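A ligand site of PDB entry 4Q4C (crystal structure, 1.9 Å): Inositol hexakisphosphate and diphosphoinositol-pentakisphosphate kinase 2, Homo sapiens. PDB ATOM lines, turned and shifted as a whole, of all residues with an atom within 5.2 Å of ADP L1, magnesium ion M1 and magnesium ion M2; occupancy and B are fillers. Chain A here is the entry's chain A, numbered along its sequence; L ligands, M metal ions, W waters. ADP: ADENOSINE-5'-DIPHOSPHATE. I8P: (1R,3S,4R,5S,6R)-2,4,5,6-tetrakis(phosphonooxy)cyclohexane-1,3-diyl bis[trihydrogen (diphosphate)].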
ATOM      1  N   ARG A  98       3.747  13.636 -17.700  1.00  0.00           N
ATOM      2  CA  ARG A  98       2.657  13.721 -16.707  1.00  0.00           C
ATOM      3  C   ARG A  98       2.807  14.923 -15.763  1.00  0.00           C
ATOM      4  O   ARG A  98       1.806  15.483 -15.312  1.00  0.00           O
ATOM      5  CB  ARG A  98       2.552  12.438 -15.861  1.00  0.00           C
ATOM      6  CG  ARG A  98       1.988  11.237 -16.591  1.00  0.00           C
ATOM      7  CD  ARG A  98       1.814  10.055 -15.637  1.00  0.00           C
ATOM      8  NE  ARG A  98       1.956   8.792 -16.365  1.00  0.00           N
ATOM      9  CZ  ARG A  98       1.011   8.222 -17.110  1.00  0.00           C
ATOM     10  NH1 ARG A  98      -0.189   8.762 -17.230  1.00  0.00           N
ATOM     11  NH2 ARG A  98       1.268   7.091 -17.742  1.00  0.00           N
ATOM     12  N   PRO A 113      -6.081  14.383  -8.426  1.00  0.00           N
ATOM     13  CA  PRO A 113      -5.613  13.810  -7.170  1.00  0.00           C
ATOM     14  C   PRO A 113      -4.463  14.610  -6.555  1.00  0.00           C
ATOM     15  O   PRO A 113      -3.624  15.118  -7.280  1.00  0.00           O
ATOM     16  CB  PRO A 113      -5.127  12.405  -7.583  1.00  0.00           C
ATOM     17  CG  PRO A 113      -5.812  12.124  -8.881  1.00  0.00           C
ATOM     18  CD  PRO A 113      -5.927  13.451  -9.559  1.00  0.00           C
ATOM     19  N   VAL A 149      -1.024   5.668  -5.733  1.00  0.00           N
ATOM     20  CA  VAL A 149      -0.752   5.362  -7.119  1.00  0.00           C
ATOM     21  C   VAL A 149       0.634   5.942  -7.473  1.00  0.00           C
ATOM     22  O   VAL A 149       0.992   7.036  -7.033  1.00  0.00           O
ATOM     23  CB  VAL A 149      -1.858   5.944  -8.030  1.00  0.00           C
ATOM     24  CG1 VAL A 149      -1.665   5.510  -9.476  1.00  0.00           C
ATOM     25  CG2 VAL A 149      -3.226   5.497  -7.558  1.00  0.00           C
ATOM     26  N   LYS A 151       2.983   6.629 -10.844  1.00  0.00           N
ATOM     27  CA  LYS A 151       2.967   6.758 -12.303  1.00  0.00           C
ATOM     28  C   LYS A 151       4.328   7.221 -12.813  1.00  0.00           C
ATOM     29  O   LYS A 151       4.905   8.175 -12.295  1.00  0.00           O
ATOM     30  CB  LYS A 151       1.911   7.765 -12.779  1.00  0.00           C
ATOM     31  CG  LYS A 151       0.501   7.500 -12.238  1.00  0.00           C
ATOM     32  CD  LYS A 151      -0.535   8.475 -12.788  1.00  0.00           C
ATOM     33  CE  LYS A 151      -1.916   8.192 -12.211  1.00  0.00           C
ATOM     34  NZ  LYS A 151      -2.954   9.173 -12.690  1.00  0.00           N
ATOM     35  N   ALA A 155       4.273  10.113 -19.769  1.00  0.00           N
ATOM     36  CA  ALA A 155       2.882   9.768 -20.034  1.00  0.00           C
ATOM     37  C   ALA A 155       2.714   8.639 -21.048  1.00  0.00           C
ATOM     38  O   ALA A 155       1.655   8.038 -21.173  1.00  0.00           O
ATOM     39  CB  ALA A 155       2.126  10.984 -20.511  1.00  0.00           C
ATOM     40  N   ASP A 157       4.543   5.944 -20.871  1.00  0.00           N
ATOM     41  CA  ASP A 157       4.821   4.712 -20.114  1.00  0.00           C
ATOM     42  C   ASP A 157       3.586   4.365 -19.245  1.00  0.00           C
ATOM     43  O   ASP A 157       3.257   5.092 -18.309  1.00  0.00           O
ATOM     44  CB  ASP A 157       6.083   4.910 -19.284  1.00  0.00           C
ATOM     45  CG  ASP A 157       6.499   3.664 -18.497  1.00  0.00           C
ATOM     46  OD1 ASP A 157       5.669   2.772 -18.231  1.00  0.00           O
ATOM     47  OD2 ASP A 157       7.681   3.622 -18.066  1.00  0.00           O
ATOM     48  N   HIS A 158       2.911   3.284 -19.595  1.00  0.00           N
ATOM     49  CA  HIS A 158       1.644   2.895 -18.972  1.00  0.00           C
ATOM     50  C   HIS A 158       1.788   1.904 -17.819  1.00  0.00           C
ATOM     51  O   HIS A 158       0.810   1.326 -17.363  1.00  0.00           O
ATOM     52  CB  HIS A 158       0.714   2.387 -20.068  1.00  0.00           C
ATOM     53  CG  HIS A 158       0.510   3.407 -21.133  1.00  0.00           C
ATOM     54  ND1 HIS A 158      -0.223   4.550 -20.916  1.00  0.00           N
ATOM     55  CD2 HIS A 158       1.055   3.538 -22.353  1.00  0.00           C
ATOM     56  CE1 HIS A 158      -0.159   5.323 -21.986  1.00  0.00           C
ATOM     57  NE2 HIS A 158       0.613   4.722 -22.877  1.00  0.00           N
ATOM     58  N   VAL A 160       1.698   1.777 -14.588  1.00  0.00           N
ATOM     59  CA  VAL A 160       1.170   2.465 -13.412  1.00  0.00           C
ATOM     60  C   VAL A 160       0.943   1.412 -12.355  1.00  0.00           C
ATOM     61  O   VAL A 160       0.309   0.384 -12.624  1.00  0.00           O
ATOM     62  CB  VAL A 160      -0.143   3.180 -13.768  1.00  0.00           C
ATOM     63  CG1 VAL A 160      -0.857   3.713 -12.531  1.00  0.00           C
ATOM     64  CG2 VAL A 160       0.136   4.312 -14.735  1.00  0.00           C
ATOM     65  N   ILE A 162      -0.410   0.478  -8.309  1.00  0.00           N
ATOM     66  CA  ILE A 162      -1.230   0.840  -7.151  1.00  0.00           C
ATOM     67  C   ILE A 162      -0.747  -0.011  -5.991  1.00  0.00           C
ATOM     68  O   ILE A 162      -0.553  -1.210  -6.143  1.00  0.00           O
ATOM     69  CB  ILE A 162      -2.718   0.638  -7.459  1.00  0.00           C
ATOM     70  CG1 ILE A 162      -3.034   1.409  -8.757  1.00  0.00           C
ATOM     71  CG2 ILE A 162      -3.587   1.041  -6.247  1.00  0.00           C
ATOM     72  CD1 ILE A 162      -4.478   1.546  -9.130  1.00  0.00           C
ATOM     73  N   LEU A 175      -0.438  -2.123 -13.610  1.00  0.00           N
ATOM     74  CA  LEU A 175      -1.178  -1.842 -14.823  1.00  0.00           C
ATOM     75  C   LEU A 175      -0.244  -1.755 -16.024  1.00  0.00           C
ATOM     76  O   LEU A 175       0.939  -1.483 -15.912  1.00  0.00           O
ATOM     77  CB  LEU A 175      -2.013  -0.539 -14.687  1.00  0.00           C
ATOM     78  CG  LEU A 175      -3.222  -0.541 -13.742  1.00  0.00           C
ATOM     79  CD1 LEU A 175      -2.904  -1.071 -12.360  1.00  0.00           C
ATOM     80  CD2 LEU A 175      -3.829   0.852 -13.601  1.00  0.00           C
ATOM     81  N   ARG A 177      -0.358  -1.450 -20.748  1.00  0.00           N
ATOM     82  CA  ARG A 177      -1.114  -1.528 -21.990  1.00  0.00           C
ATOM     83  C   ARG A 177      -1.714  -2.927 -22.148  1.00  0.00           C
ATOM     84  O   ARG A 177      -1.008  -3.937 -22.038  1.00  0.00           O
ATOM     85  CB  ARG A 177      -0.217  -1.252 -23.200  1.00  0.00           C
ATOM     86  CG  ARG A 177      -0.119   0.196 -23.572  1.00  0.00           C
ATOM     87  CD  ARG A 177      -1.336   0.596 -24.412  1.00  0.00           C
ATOM     88  NE  ARG A 177      -1.437   2.044 -24.580  1.00  0.00           N
ATOM     89  CZ  ARG A 177      -2.146   2.862 -23.778  1.00  0.00           C
ATOM     90  NH1 ARG A 177      -2.816   2.387 -22.719  1.00  0.00           N
ATOM     91  NH2 ARG A 177      -2.169   4.171 -24.037  1.00  0.00           N
ATOM     92  N   GLU A 201       0.447   9.717  -6.090  1.00  0.00           N
ATOM     93  CA  GLU A 201      -0.822  10.410  -5.865  1.00  0.00           C
ATOM     94  C   GLU A 201      -1.798   9.596  -5.052  1.00  0.00           C
ATOM     95  O   GLU A 201      -1.713   8.345  -5.003  1.00  0.00           O
ATOM     96  CB  GLU A 201      -1.451  10.848  -7.177  1.00  0.00           C
ATOM     97  CG  GLU A 201      -1.833   9.717  -8.085  1.00  0.00           C
ATOM     98  CD  GLU A 201      -2.242  10.204  -9.473  1.00  0.00           C
ATOM     99  OE1 GLU A 201      -3.365   9.865  -9.889  1.00  0.00           O
ATOM    100  OE2 GLU A 201      -1.451  10.892 -10.137  1.00  0.00           O
ATOM    101  N   GLU A 202      -2.683  10.311  -4.366  1.00  0.00           N
ATOM    102  CA  GLU A 202      -3.713   9.670  -3.559  1.00  0.00           C
ATOM    103  C   GLU A 202      -4.609   8.858  -4.480  1.00  0.00           C
ATOM    104  O   GLU A 202      -4.840   9.246  -5.633  1.00  0.00           O
ATOM    105  CB  GLU A 202      -4.550  10.675  -2.771  1.00  0.00           C
ATOM    106  CG  GLU A 202      -5.251  11.687  -3.654  1.00  0.00           C
ATOM    107  CD  GLU A 202      -6.267  12.584  -2.918  1.00  0.00           C
ATOM    108  OE1 GLU A 202      -6.787  12.152  -1.842  1.00  0.00           O
ATOM    109  OE2 GLU A 202      -6.533  13.702  -3.433  1.00  0.00           O
ATOM    110  N   PHE A 203      -5.045   7.709  -3.967  1.00  0.00           N
ATOM    111  CA  PHE A 203      -6.012   6.840  -4.635  1.00  0.00           C
ATOM    112  C   PHE A 203      -7.422   7.389  -4.403  1.00  0.00           C
ATOM    113  O   PHE A 203      -7.838   7.594  -3.250  1.00  0.00           O
ATOM    114  CB  PHE A 203      -5.909   5.413  -4.090  1.00  0.00           C
ATOM    115  CG  PHE A 203      -6.834   4.431  -4.762  1.00  0.00           C
ATOM    116  CD1 PHE A 203      -6.478   3.842  -5.948  1.00  0.00           C
ATOM    117  CD2 PHE A 203      -8.063   4.094  -4.189  1.00  0.00           C
ATOM    118  CE1 PHE A 203      -7.318   2.936  -6.574  1.00  0.00           C
ATOM    119  CE2 PHE A 203      -8.923   3.202  -4.819  1.00  0.00           C
ATOM    120  CZ  PHE A 203      -8.546   2.620  -6.007  1.00  0.00           C
ATOM    121  N   MET A 204      -8.139   7.602  -5.502  1.00  0.00           N
ATOM    122  CA  MET A 204      -9.491   8.154  -5.474  1.00  0.00           C
ATOM    123  C   MET A 204     -10.445   6.955  -5.573  1.00  0.00           C
ATOM    124  O   MET A 204     -10.420   6.234  -6.569  1.00  0.00           O
ATOM    125  CB  MET A 204      -9.708   9.086  -6.649  1.00  0.00           C
ATOM    126  CG  MET A 204      -8.681  10.213  -6.838  1.00  0.00           C
ATOM    127  SD  MET A 204      -8.273  11.105  -5.322  1.00  0.00           S
ATOM    128  CE  MET A 204      -9.773  12.071  -5.062  1.00  0.00           C
ATOM    129  N   ASP A 210     -13.695   3.641 -14.597  1.00  0.00           N
ATOM    130  CA  ASP A 210     -13.100   4.875 -15.134  1.00  0.00           C
ATOM    131  C   ASP A 210     -14.132   5.547 -16.044  1.00  0.00           C
ATOM    132  O   ASP A 210     -14.849   4.845 -16.767  1.00  0.00           O
ATOM    133  CB  ASP A 210     -11.925   4.569 -16.077  1.00  0.00           C
ATOM    134  CG  ASP A 210     -10.776   3.908 -15.410  1.00  0.00           C
ATOM    135  OD1 ASP A 210     -10.693   3.954 -14.162  1.00  0.00           O
ATOM    136  OD2 ASP A 210      -9.945   3.317 -16.159  1.00  0.00           O
ATOM    137  N   LYS A 212     -14.174   7.699 -19.389  1.00  0.00           N
ATOM    138  CA  LYS A 212     -13.354   8.148 -20.494  1.00  0.00           C
ATOM    139  C   LYS A 212     -14.137   9.250 -21.222  1.00  0.00           C
ATOM    140  O   LYS A 212     -15.276   9.043 -21.642  1.00  0.00           O
ATOM    141  CB  LYS A 212     -13.064   7.001 -21.465  1.00  0.00           C
ATOM    142  CG  LYS A 212     -12.345   5.780 -20.881  1.00  0.00           C
ATOM    143  CD  LYS A 212     -10.892   6.022 -20.588  1.00  0.00           C
ATOM    144  CE  LYS A 212      -9.954   6.013 -21.823  1.00  0.00           C
ATOM    145  NZ  LYS A 212      -8.568   6.381 -21.393  1.00  0.00           N
ATOM    146  N   ARG A 226     -15.718   2.331 -18.243  1.00  0.00           N
ATOM    147  CA  ARG A 226     -15.202   0.964 -18.324  1.00  0.00           C
ATOM    148  C   ARG A 226     -14.669   0.550 -16.961  1.00  0.00           C
ATOM    149  O   ARG A 226     -14.328   1.395 -16.125  1.00  0.00           O
ATOM    150  CB  ARG A 226     -14.131   0.809 -19.429  1.00  0.00           C
ATOM    151  CG  ARG A 226     -12.943   1.741 -19.321  1.00  0.00           C
ATOM    152  CD  ARG A 226     -11.717   1.046 -18.738  1.00  0.00           C
ATOM    153  NE  ARG A 226     -10.555   1.951 -18.715  1.00  0.00           N
ATOM    154  CZ  ARG A 226      -9.725   2.167 -19.722  1.00  0.00           C
ATOM    155  NH1 ARG A 226      -9.882   1.548 -20.903  1.00  0.00           N
ATOM    156  NH2 ARG A 226      -8.722   3.006 -19.560  1.00  0.00           N
ATOM    157  N   SER A 228     -12.536  -0.495 -14.007  1.00  0.00           N
ATOM    158  CA  SER A 228     -11.233   0.002 -13.588  1.00  0.00           C
ATOM    159  C   SER A 228     -10.222  -1.113 -13.860  1.00  0.00           C
ATOM    160  O   SER A 228     -10.414  -2.223 -13.374  1.00  0.00           O
ATOM    161  CB  SER A 228     -11.190   0.312 -12.068  1.00  0.00           C
ATOM    162  OG  SER A 228     -12.342   1.020 -11.629  1.00  0.00           O
ATOM    163  N   PRO A 229      -9.163  -0.808 -14.623  1.00  0.00           N
ATOM    164  CA  PRO A 229      -8.203  -1.835 -15.022  1.00  0.00           C
ATOM    165  C   PRO A 229      -7.501  -2.505 -13.866  1.00  0.00           C
ATOM    166  O   PRO A 229      -7.025  -3.636 -14.016  1.00  0.00           O
ATOM    167  CB  PRO A 229      -7.187  -1.099 -15.920  1.00  0.00           C
ATOM    168  CG  PRO A 229      -7.600   0.326 -15.954  1.00  0.00           C
ATOM    169  CD  PRO A 229      -8.964   0.453 -15.362  1.00  0.00           C
ATOM    170  N   ASP A 273      -9.316  11.229 -18.794  1.00  0.00           N
ATOM    171  CA  ASP A 273      -9.944  10.256 -17.904  1.00  0.00           C
ATOM    172  C   ASP A 273     -10.416  10.971 -16.637  1.00  0.00           C
ATOM    173  O   ASP A 273      -9.673  11.827 -16.082  1.00  0.00           O
ATOM    174  CB  ASP A 273      -8.980   9.145 -17.535  1.00  0.00           C
ATOM    175  CG  ASP A 273      -8.416   8.403 -18.753  1.00  0.00           C
ATOM    176  OD1 ASP A 273      -8.983   8.474 -19.876  1.00  0.00           O
ATOM    177  OD2 ASP A 273      -7.374   7.736 -18.609  1.00  0.00           O
ATOM    178  N   LEU A 275     -12.160  10.350 -12.699  1.00  0.00           N
ATOM    179  CA  LEU A 275     -12.480   9.504 -11.562  1.00  0.00           C
ATOM    180  C   LEU A 275     -13.584  10.172 -10.779  1.00  0.00           C
ATOM    181  O   LEU A 275     -13.420  11.284 -10.215  1.00  0.00           O
ATOM    182  CB  LEU A 275     -11.248   9.262 -10.670  1.00  0.00           C
ATOM    183  CG  LEU A 275      -9.997   8.787 -11.393  1.00  0.00           C
ATOM    184  CD1 LEU A 275      -8.783   8.689 -10.483  1.00  0.00           C
ATOM    185  CD2 LEU A 275     -10.292   7.472 -12.071  1.00  0.00           C
ATOM    186  N   CYS A 284      -7.366  12.452 -14.093  1.00  0.00           N
ATOM    187  CA  CYS A 284      -6.126  11.721 -13.760  1.00  0.00           C
ATOM    188  C   CYS A 284      -5.179  11.464 -14.941  1.00  0.00           C
ATOM    189  O   CYS A 284      -4.058  10.958 -14.723  1.00  0.00           O
ATOM    190  CB  CYS A 284      -6.435  10.374 -13.073  1.00  0.00           C
ATOM    191  SG  CYS A 284      -7.125   9.100 -14.163  1.00  0.00           S
ATOM    192  N   ASP A 285      -5.579  11.884 -16.146  1.00  0.00           N
ATOM    193  CA  ASP A 285      -4.856  11.547 -17.361  1.00  0.00           C
ATOM    194  C   ASP A 285      -5.455  12.394 -18.474  1.00  0.00           C
ATOM    195  O   ASP A 285      -6.674  12.505 -18.567  1.00  0.00           O
ATOM    196  CB  ASP A 285      -5.031  10.051 -17.650  1.00  0.00           C
ATOM    197  CG  ASP A 285      -4.138   9.493 -18.783  1.00  0.00           C
ATOM    198  OD1 ASP A 285      -3.075  10.046 -19.127  1.00  0.00           O
ATOM    199  OD2 ASP A 285      -4.519   8.423 -19.337  1.00  0.00           O
ATOM    200  N   VAL A 286      -4.593  13.055 -19.246  1.00  0.00           N
ATOM    201  CA  VAL A 286      -5.009  13.789 -20.448  1.00  0.00           C
ATOM    202  C   VAL A 286      -4.167  13.245 -21.579  1.00  0.00           C
ATOM    203  O   VAL A 286      -2.934  13.407 -21.586  1.00  0.00           O
ATOM    204  CB  VAL A 286      -4.767  15.306 -20.326  1.00  0.00           C
ATOM    205  CG1 VAL A 286      -5.163  16.051 -21.604  1.00  0.00           C
ATOM    206  CG2 VAL A 286      -5.542  15.845 -19.138  1.00  0.00           C
ATOM    207  N   ASN A 287      -4.823  12.589 -22.521  1.00  0.00           N
ATOM    208  CA  ASN A 287      -4.109  11.930 -23.613  1.00  0.00           C
ATOM    209  C   ASN A 287      -4.004  12.697 -24.934  1.00  0.00           C
ATOM    210  O   ASN A 287      -3.199  12.322 -25.791  1.00  0.00           O
ATOM    211  CB  ASN A 287      -4.750  10.575 -23.831  1.00  0.00           C
ATOM    212  CG  ASN A 287      -4.631   9.697 -22.612  1.00  0.00           C
ATOM    213  OD1 ASN A 287      -3.519   9.466 -22.108  1.00  0.00           O
ATOM    214  ND2 ASN A 287      -5.751   9.199 -22.129  1.00  0.00           N
HETATM  215  PB  ADP L   1      -2.396   5.955 -18.417  1.00  0.00           P
HETATM  216  O1B ADP L   1      -1.867   7.260 -18.983  1.00  0.00           O
HETATM  217  O2B ADP L   1      -1.385   4.863 -18.407  1.00  0.00           O
HETATM  218  O3B ADP L   1      -3.747   5.556 -18.991  1.00  0.00           O
HETATM  219  PA  ADP L   1      -3.780   6.757 -15.988  1.00  0.00           P
HETATM  220  O1A ADP L   1      -3.365   7.928 -15.124  1.00  0.00           O
HETATM  221  O2A ADP L   1      -5.024   6.853 -16.795  1.00  0.00           O
HETATM  222  O3A ADP L   1      -2.515   6.225 -16.824  1.00  0.00           O
HETATM  223  O5' ADP L   1      -3.918   5.531 -14.947  1.00  0.00           O
HETATM  224  C5' ADP L   1      -4.369   4.245 -15.384  1.00  0.00           C
HETATM  225  C4' ADP L   1      -5.601   3.829 -14.593  1.00  0.00           C
HETATM  226  O4' ADP L   1      -5.274   3.737 -13.211  1.00  0.00           O
HETATM  227  C3' ADP L   1      -6.756   4.805 -14.627  1.00  0.00           C
HETATM  228  O3' ADP L   1      -7.625   4.655 -15.756  1.00  0.00           O
HETATM  229  C2' ADP L   1      -7.488   4.509 -13.330  1.00  0.00           C
HETATM  230  O2' ADP L   1      -8.299   3.301 -13.368  1.00  0.00           O
HETATM  231  C1' ADP L   1      -6.338   4.232 -12.390  1.00  0.00           C
HETATM  232  N9  ADP L   1      -5.873   5.439 -11.674  1.00  0.00           N
HETATM  233  C8  ADP L   1      -4.948   6.346 -12.050  1.00  0.00           C
HETATM  234  N7  ADP L   1      -4.784   7.309 -11.094  1.00  0.00           N
HETATM  235  C5  ADP L   1      -5.649   6.994 -10.108  1.00  0.00           C
HETATM  236  C6  ADP L   1      -5.989   7.547  -8.789  1.00  0.00           C
HETATM  237  N6  ADP L   1      -5.383   8.664  -8.360  1.00  0.00           N
HETATM  238  N1  ADP L   1      -6.929   6.931  -8.056  1.00  0.00           N
HETATM  239  C2  ADP L   1      -7.535   5.815  -8.485  1.00  0.00           C
HETATM  240  N3  ADP L   1      -7.280   5.253  -9.678  1.00  0.00           N
HETATM  241  C4  ADP L   1      -6.344   5.777 -10.490  1.00  0.00           C
HETATM  242  C1  I8P L   2      -5.464   4.114 -25.790  1.00  0.00           C
HETATM  243  C2  I8P L   2      -4.567   4.508 -26.986  1.00  0.00           C
HETATM  244  C3  I8P L   2      -3.533   3.393 -27.224  1.00  0.00           C
HETATM  245  C4  I8P L   2      -4.243   2.086 -27.595  1.00  0.00           C
HETATM  246  C5  I8P L   2      -5.244   1.679 -26.501  1.00  0.00           C
HETATM  247  C6  I8P L   2      -6.227   2.796 -26.078  1.00  0.00           C
HETATM  248  O11 I8P L   2      -6.411   5.154 -25.547  1.00  0.00           O
HETATM  249  O12 I8P L   2      -5.398   4.645 -28.138  1.00  0.00           O
HETATM  250  O13 I8P L   2      -2.572   3.781 -28.240  1.00  0.00           O
HETATM  251  O14 I8P L   2      -3.312   1.005 -27.624  1.00  0.00           O
HETATM  252  O15 I8P L   2      -6.036   0.600 -26.985  1.00  0.00           O
HETATM  253  O16 I8P L   2      -6.846   2.320 -24.856  1.00  0.00           O
HETATM  254  O21 I8P L   2      -7.402   6.698 -23.884  1.00  0.00           O
HETATM  255  O22 I8P L   2      -5.622   7.172 -27.704  1.00  0.00           O
HETATM  256  O23 I8P L   2      -0.513   2.750 -27.387  1.00  0.00           O
HETATM  257  O24 I8P L   2      -1.178   1.036 -29.026  1.00  0.00           O
HETATM  258  O25 I8P L   2      -5.243  -1.683 -27.760  1.00  0.00           O
HETATM  259  O26 I8P L   2      -8.993   1.833 -25.973  1.00  0.00           O
HETATM  260  O31 I8P L   2      -5.423   7.330 -25.331  1.00  0.00           O
HETATM  261  O32 I8P L   2      -6.797   6.041 -29.531  1.00  0.00           O
HETATM  262  O33 I8P L   2      -0.444   4.577 -29.092  1.00  0.00           O
HETATM  263  O34 I8P L   2      -3.469   0.651 -30.109  1.00  0.00           O
HETATM  264  O35 I8P L   2      -4.877  -1.004 -25.303  1.00  0.00           O
HETATM  265  O36 I8P L   2      -8.783   3.595 -24.158  1.00  0.00           O
HETATM  266  O41 I8P L   2      -5.011   5.729 -23.429  1.00  0.00           O
HETATM  267  O42 I8P L   2      -4.355   6.237 -29.579  1.00  0.00           O
HETATM  268  O43 I8P L   2      -1.146   5.028 -26.707  1.00  0.00           O
HETATM  269  O44 I8P L   2      -2.385  -1.079 -28.610  1.00  0.00           O
HETATM  270  O45 I8P L   2      -7.218  -1.423 -26.201  1.00  0.00           O
HETATM  271  O46 I8P L   2      -8.606   1.230 -23.576  1.00  0.00           O
HETATM  272  O51 I8P L   2      -5.944   6.336 -20.879  1.00  0.00           O
HETATM  273  O55 I8P L   2      -9.348  -2.731 -26.006  1.00  0.00           O
HETATM  274  O61 I8P L   2      -3.312   6.694 -21.581  1.00  0.00           O
HETATM  275  O65 I8P L   2      -7.222  -3.900 -26.729  1.00  0.00           O
HETATM  276  O71 I8P L   2      -4.423   4.296 -21.381  1.00  0.00           O
HETATM  277  O75 I8P L   2      -8.344  -2.286 -28.316  1.00  0.00           O
HETATM  278  PA1 I8P L   2      -6.084   6.333 -24.463  1.00  0.00           P
HETATM  279  PA2 I8P L   2      -5.570   6.135 -28.793  1.00  0.00           P
HETATM  280  PA3 I8P L   2      -1.032   4.052 -27.827  1.00  0.00           P
HETATM  281  PA4 I8P L   2      -2.638   0.335 -28.942  1.00  0.00           P
HETATM  282  PA5 I8P L   2      -5.704  -0.969 -26.548  1.00  0.00           P
HETATM  283  PA6 I8P L   2      -8.469   2.229 -24.659  1.00  0.00           P
HETATM  284  PB1 I8P L   2      -4.701   5.750 -21.769  1.00  0.00           P
HETATM  285  PB5 I8P L   2      -7.994  -2.664 -26.913  1.00  0.00           P
HETATM  286 MG    MG M   1      -2.679   8.344 -20.578  1.00  0.00          MG
HETATM  287 MG    MG M   2      -5.641   6.627 -18.752  1.00  0.00          MG
HETATM  288  O   HOH W   1      -4.222   1.459 -17.476  1.00  0.00           O
HETATM  289  O   HOH W   2      -0.950   8.860 -21.348  1.00  0.00           O
HETATM  290  O   HOH W   3      -6.859   4.940 -18.370  1.00  0.00           O
HETATM  291  O   HOH W   4      -9.433   3.389  -9.824  1.00  0.00           O
HETATM  292  O   HOH W   5      -1.788   2.521 -17.169  1.00  0.00           O
HETATM  293  O   HOH W   6      -7.977   0.842 -12.088  1.00  0.00           O
HETATM  294  O   HOH W   7      -5.363   2.817 -19.253  1.00  0.00           O
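Residues that only touch magnesium ion M2: Lys 212. Within 4 Å of magnesium ion M2: Lys 212, Asp 273 and Asp 285.
Magnesium ion M1 is bound by water W2, 2.0 Å away. O61 of I8P L2 binds magnesium ion M1 (2.0 Å). OD1 of Asn 287 binds magnesium ion M1 (2.1 Å). Magnesium ion M1 is bound by O1B of ADP L1 (2.1 Å). OD2 of Asp 285 is bound to magnesium ion M1. OD1 of Asp 285 is bound to magnesium ion M1 (2.3 Å). Magnesium ion M1 has six donor atoms within binding distance.
The nearest printed residue that does not touch magnesium ion M1 is His 158 (4.2 Å).
OD1 of Asp 273 lies within salt-bridge range of NZ of Lys 212. The backbone NH of Cys 284 lies within hydrogen-bond range of the backbone carbonyl oxygen of Asp 273, at 3.1 Å. NZ of Lys 151 is in salt-bridge range of OE1 of Glu 201 (2.9 Å). The backbone carbonyl oxygen of Asp 157 sits at hydrogen-bond distance from the guanidinium group of Arg 98, at 2.9 Å. OD1 of Asp 285 sits close to NH1 of Arg 98 (3.7 Å). The backbone carbonyl oxygen (O) of Val 160 is in hydrogen-bond range of the backbone NH (N) of Leu 175, 2.8 Å away. The side-chain carboxylate (OD2) of Asp 210 lies within salt-bridge range of the guanidinium group (NE) of Arg 226, 3.0 Å away. NZ of Lys 151 is in hydrogen-bond range of O of Cys 284, at 2.9 Å.
The side-chain carboxylate (OE1) of Glu 201 sits at hydrogen-bond distance from a nitrogen (N6) of ADP L1. The backbone carbonyl oxygen (O) of Glu 202 lies within hydrogen-bond range of a nitrogen (N6) of ADP L1 (2.8 Å). An oxygen (O46) of I8P L2 is in salt-bridge range of the guanidinium group (NH1) of Arg 226. NH2 of Arg 98 lies within salt-bridge range of O2B of ADP L1 (3.5 Å). An oxygen (O2B) of ADP L1 is in hydrogen-bond range of a ring nitrogen (ND1) of His 158. The backbone NH of Met 204 sits at hydrogen-bond distance from a nitrogen (N1) of ADP L1. The side-chain amino group (NZ) of Lys 151 lies within salt-bridge range of an oxygen (O1A) of ADP L1 (2.8 Å). O2' of ADP L1 is in hydrogen-bond range of OD1 of Asp 210, at 2.6 Å. NH1 of Arg 177 is in salt-bridge range of O71 of I8P L2, at 2.8 Å. NZ of Lys 212 lies within salt-bridge range of O21 of I8P L2, 2.8 Å away.
Magnesium ion M2 is bound by the side-chain carboxylate of Asp 273 (2.1 Å), an oxygen (O2A) of ADP L1 (2.1 Å), water W3 (2.1 Å), an oxygen (O51) of I8P L2 (2.2 Å), an oxygen (O3B) of ADP L1 (2.2 Å) and the side-chain carboxylate of Asp 285 (2.2 Å).
Water W3 lies within hydrogen-bond range of an oxygen (O3') of ADP L1 (2.7 Å) and the guanidinium group (NH2) of Arg 226 (2.9 Å). Water W5 bridges an oxygen (O2B) of ADP L1 and the backbone carbonyl oxygen of His 158. Water W7 bridges O71 of I8P L2 and NH2 of Arg 226.
The backbone carbonyl oxygen (O) of Cys 284 lies close to an oxygen (O1A) of ADP L1, at 3.1 Å. Merely in contact with ADP L1: Pro 113, Val 149, Val 160, Leu 175, Phe 203, Pro 229 and Leu 275. Of the 26 residues printed, 17 come within 4 Å of ADP L1. The nearest printed residue that does not touch ADP L1 is Asn 287 (4.2 Å).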
